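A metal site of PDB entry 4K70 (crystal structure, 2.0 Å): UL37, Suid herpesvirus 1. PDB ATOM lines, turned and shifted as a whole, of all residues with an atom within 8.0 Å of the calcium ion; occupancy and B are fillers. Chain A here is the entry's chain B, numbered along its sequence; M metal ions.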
ATOM      1  N   VAL A 380     -10.312 -29.506 -26.780  1.00  0.00           N
ATOM      2  CA  VAL A 380     -10.337 -28.185 -27.395  1.00  0.00           C
ATOM      3  C   VAL A 380      -9.079 -27.408 -26.935  1.00  0.00           C
ATOM      4  O   VAL A 380      -8.385 -26.793 -27.748  1.00  0.00           O
ATOM      5  CB  VAL A 380     -11.621 -27.405 -27.070  1.00  0.00           C
ATOM      6  CG1 VAL A 380     -11.574 -26.016 -27.688  1.00  0.00           C
ATOM      7  CG2 VAL A 380     -12.846 -28.164 -27.573  1.00  0.00           C
ATOM      8  N   VAL A 381      -8.787 -27.483 -25.639  1.00  0.00           N
ATOM      9  CA  VAL A 381      -7.569 -26.876 -25.093  1.00  0.00           C
ATOM     10  C   VAL A 381      -6.316 -27.359 -25.823  1.00  0.00           C
ATOM     11  O   VAL A 381      -5.472 -26.551 -26.197  1.00  0.00           O
ATOM     12  CB  VAL A 381      -7.419 -27.165 -23.567  1.00  0.00           C
ATOM     13  CG1 VAL A 381      -6.036 -26.817 -23.060  1.00  0.00           C
ATOM     14  CG2 VAL A 381      -8.483 -26.389 -22.790  1.00  0.00           C
ATOM     15  N   HIS A 382      -6.192 -28.675 -26.013  1.00  0.00           N
ATOM     16  CA  HIS A 382      -5.010 -29.260 -26.643  1.00  0.00           C
ATOM     17  C   HIS A 382      -4.871 -28.818 -28.089  1.00  0.00           C
ATOM     18  O   HIS A 382      -3.754 -28.670 -28.579  1.00  0.00           O
ATOM     19  CB  HIS A 382      -5.043 -30.799 -26.572  1.00  0.00           C
ATOM     20  CG  HIS A 382      -4.524 -31.362 -25.288  1.00  0.00           C
ATOM     21  ND1 HIS A 382      -3.190 -31.297 -24.939  1.00  0.00           N
ATOM     22  CD2 HIS A 382      -5.139 -32.028 -24.280  1.00  0.00           C
ATOM     23  CE1 HIS A 382      -3.020 -31.867 -23.756  1.00  0.00           C
ATOM     24  NE2 HIS A 382      -4.185 -32.329 -23.341  1.00  0.00           N
ATOM     25  N   ARG A 383      -6.000 -28.601 -28.755  1.00  0.00           N
ATOM     26  CA  ARG A 383      -5.995 -28.100 -30.140  1.00  0.00           C
ATOM     27  C   ARG A 383      -5.521 -26.662 -30.225  1.00  0.00           C
ATOM     28  O   ARG A 383      -4.882 -26.270 -31.203  1.00  0.00           O
ATOM     29  CB  ARG A 383      -7.404 -28.124 -30.737  1.00  0.00           C
ATOM     30  CG  ARG A 383      -7.929 -29.498 -31.123  1.00  0.00           C
ATOM     31  CD  ARG A 383      -8.999 -29.346 -32.168  1.00  0.00           C
ATOM     32  NE  ARG A 383     -10.352 -29.224 -31.651  1.00  0.00           N
ATOM     33  CZ  ARG A 383     -11.287 -28.474 -32.238  1.00  0.00           C
ATOM     34  NH1 ARG A 383     -10.991 -27.759 -33.325  1.00  0.00           N
ATOM     35  NH2 ARG A 383     -12.517 -28.425 -31.744  1.00  0.00           N
ATOM     36  N   LEU A 384      -5.870 -25.858 -29.235  1.00  0.00           N
ATOM     37  CA  LEU A 384      -5.533 -24.436 -29.238  1.00  0.00           C
ATOM     38  C   LEU A 384      -4.097 -24.159 -28.817  1.00  0.00           C
ATOM     39  O   LEU A 384      -3.503 -23.155 -29.205  1.00  0.00           O
ATOM     40  CB  LEU A 384      -6.461 -23.657 -28.303  1.00  0.00           C
ATOM     41  CG  LEU A 384      -7.926 -23.493 -28.727  1.00  0.00           C
ATOM     42  CD1 LEU A 384      -8.761 -23.145 -27.511  1.00  0.00           C
ATOM     43  CD2 LEU A 384      -8.064 -22.427 -29.797  1.00  0.00           C
ATOM     44  N   LEU A 385      -3.557 -25.059 -28.014  1.00  0.00           N
ATOM     45  CA  LEU A 385      -2.316 -24.779 -27.298  1.00  0.00           C
ATOM     46  C   LEU A 385      -1.170 -24.475 -28.245  1.00  0.00           C
ATOM     47  O   LEU A 385      -0.370 -23.588 -27.971  1.00  0.00           O
ATOM     48  CB  LEU A 385      -1.926 -25.952 -26.395  1.00  0.00           C
ATOM     49  CG  LEU A 385      -0.618 -25.754 -25.638  1.00  0.00           C
ATOM     50  CD1 LEU A 385      -0.720 -24.545 -24.712  1.00  0.00           C
ATOM     51  CD2 LEU A 385      -0.260 -27.020 -24.868  1.00  0.00           C
ATOM     52  N   ASP A 386      -1.101 -25.202 -29.358  1.00  0.00           N
ATOM     53  CA  ASP A 386       0.042 -25.025 -30.260  1.00  0.00           C
ATOM     54  C   ASP A 386       0.063 -23.625 -30.870  1.00  0.00           C
ATOM     55  O   ASP A 386       1.121 -23.115 -31.232  1.00  0.00           O
ATOM     56  CB  ASP A 386       0.075 -26.109 -31.352  1.00  0.00           C
ATOM     57  CG  ASP A 386      -1.112 -26.044 -32.299  1.00  0.00           C
ATOM     58  OD1 ASP A 386      -1.044 -25.290 -33.284  1.00  0.00           O
ATOM     59  OD2 ASP A 386      -2.125 -26.727 -32.061  1.00  0.00           O
ATOM     60  N   ASP A 387      -1.108 -22.986 -30.938  1.00  0.00           N
ATOM     61  CA  ASP A 387      -1.227 -21.690 -31.556  1.00  0.00           C
ATOM     62  C   ASP A 387      -1.157 -20.534 -30.560  1.00  0.00           C
ATOM     63  O   ASP A 387      -1.090 -19.371 -30.974  1.00  0.00           O
ATOM     64  CB  ASP A 387      -2.552 -21.589 -32.305  1.00  0.00           C
ATOM     65  CG  ASP A 387      -2.713 -22.670 -33.359  1.00  0.00           C
ATOM     66  OD1 ASP A 387      -2.086 -22.575 -34.440  1.00  0.00           O
ATOM     67  OD2 ASP A 387      -3.476 -23.617 -33.100  1.00  0.00           O
ATOM     68  N   TYR A 388      -1.181 -20.852 -29.267  1.00  0.00           N
ATOM     69  CA  TYR A 388      -1.404 -19.835 -28.254  1.00  0.00           C
ATOM     70  C   TYR A 388      -0.380 -18.708 -28.269  1.00  0.00           C
ATOM     71  O   TYR A 388       0.830 -18.938 -28.209  1.00  0.00           O
ATOM     72  CB  TYR A 388      -1.452 -20.431 -26.854  1.00  0.00           C
ATOM     73  CG  TYR A 388      -1.951 -19.410 -25.847  1.00  0.00           C
ATOM     74  CD1 TYR A 388      -1.068 -18.523 -25.235  1.00  0.00           C
ATOM     75  CD2 TYR A 388      -3.307 -19.311 -25.566  1.00  0.00           C
ATOM     76  CE1 TYR A 388      -1.539 -17.564 -24.330  1.00  0.00           C
ATOM     77  CE2 TYR A 388      -3.779 -18.352 -24.661  1.00  0.00           C
ATOM     78  CZ  TYR A 388      -2.885 -17.487 -24.047  1.00  0.00           C
ATOM     79  OH  TYR A 388      -3.360 -16.552 -23.144  1.00  0.00           O
ATOM     80  N   TYR A 394      -3.258 -15.965 -33.409  1.00  0.00           N
ATOM     81  CA  TYR A 394      -3.973 -16.730 -32.395  1.00  0.00           C
ATOM     82  C   TYR A 394      -5.434 -16.345 -32.357  1.00  0.00           C
ATOM     83  O   TYR A 394      -6.284 -17.206 -32.149  1.00  0.00           O
ATOM     84  CB  TYR A 394      -3.353 -16.618 -30.995  1.00  0.00           C
ATOM     85  CG  TYR A 394      -4.104 -17.499 -30.001  1.00  0.00           C
ATOM     86  CD1 TYR A 394      -4.206 -18.870 -30.209  1.00  0.00           C
ATOM     87  CD2 TYR A 394      -4.723 -16.964 -28.867  1.00  0.00           C
ATOM     88  CE1 TYR A 394      -4.884 -19.695 -29.328  1.00  0.00           C
ATOM     89  CE2 TYR A 394      -5.421 -17.796 -27.967  1.00  0.00           C
ATOM     90  CZ  TYR A 394      -5.496 -19.167 -28.211  1.00  0.00           C
ATOM     91  OH  TYR A 394      -6.153 -20.026 -27.353  1.00  0.00           O
ATOM     92  N   ALA A 397      -6.827 -18.412 -35.157  1.00  0.00           N
ATOM     93  CA  ALA A 397      -6.863 -19.825 -34.793  1.00  0.00           C
ATOM     94  C   ALA A 397      -7.983 -20.120 -33.793  1.00  0.00           C
ATOM     95  O   ALA A 397      -8.719 -21.104 -33.939  1.00  0.00           O
ATOM     96  CB  ALA A 397      -5.512 -20.280 -34.258  1.00  0.00           C
ATOM     97  N   TYR A 398      -8.098 -19.280 -32.774  1.00  0.00           N
ATOM     98  CA  TYR A 398      -9.091 -19.468 -31.726  1.00  0.00           C
ATOM     99  C   TYR A 398     -10.508 -19.388 -32.302  1.00  0.00           C
ATOM    100  O   TYR A 398     -11.375 -20.209 -31.990  1.00  0.00           O
ATOM    101  CB  TYR A 398      -8.901 -18.394 -30.622  1.00  0.00           C
ATOM    102  CG  TYR A 398      -9.939 -18.498 -29.525  1.00  0.00           C
ATOM    103  CD1 TYR A 398     -11.159 -17.848 -29.653  1.00  0.00           C
ATOM    104  CD2 TYR A 398      -9.715 -19.257 -28.397  1.00  0.00           C
ATOM    105  CE1 TYR A 398     -12.129 -17.941 -28.651  1.00  0.00           C
ATOM    106  CE2 TYR A 398     -10.688 -19.374 -27.397  1.00  0.00           C
ATOM    107  CZ  TYR A 398     -11.889 -18.702 -27.528  1.00  0.00           C
ATOM    108  OH  TYR A 398     -12.862 -18.793 -26.540  1.00  0.00           O
ATOM    109  N   VAL A 401     -11.572 -22.448 -34.025  1.00  0.00           N
ATOM    110  CA  VAL A 401     -11.909 -23.520 -33.107  1.00  0.00           C
ATOM    111  C   VAL A 401     -13.281 -23.277 -32.477  1.00  0.00           C
ATOM    112  O   VAL A 401     -14.139 -24.189 -32.447  1.00  0.00           O
ATOM    113  CB  VAL A 401     -10.833 -23.673 -32.012  1.00  0.00           C
ATOM    114  CG1 VAL A 401     -11.274 -24.679 -30.966  1.00  0.00           C
ATOM    115  CG2 VAL A 401      -9.508 -24.114 -32.616  1.00  0.00           C
HETATM  116 CA    CA M   1      -3.882 -25.872 -33.304  1.00  0.00          CA
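Within 4 Å of the calcium ion: Arg 383, Asp 386 and Asp 387. The nearest printed residue that does not touch the calcium ion is Leu 384 (4.5 Å).
The calcium ion is bound by OD2 of Asp 387 (2.3 Å), OD2 of Asp 386 (2.3 Å), O of Arg 383 (2.4 Å) and OD1 of Asp 386 (2.9 Å). The calcium ion has four donor atoms within binding distance.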
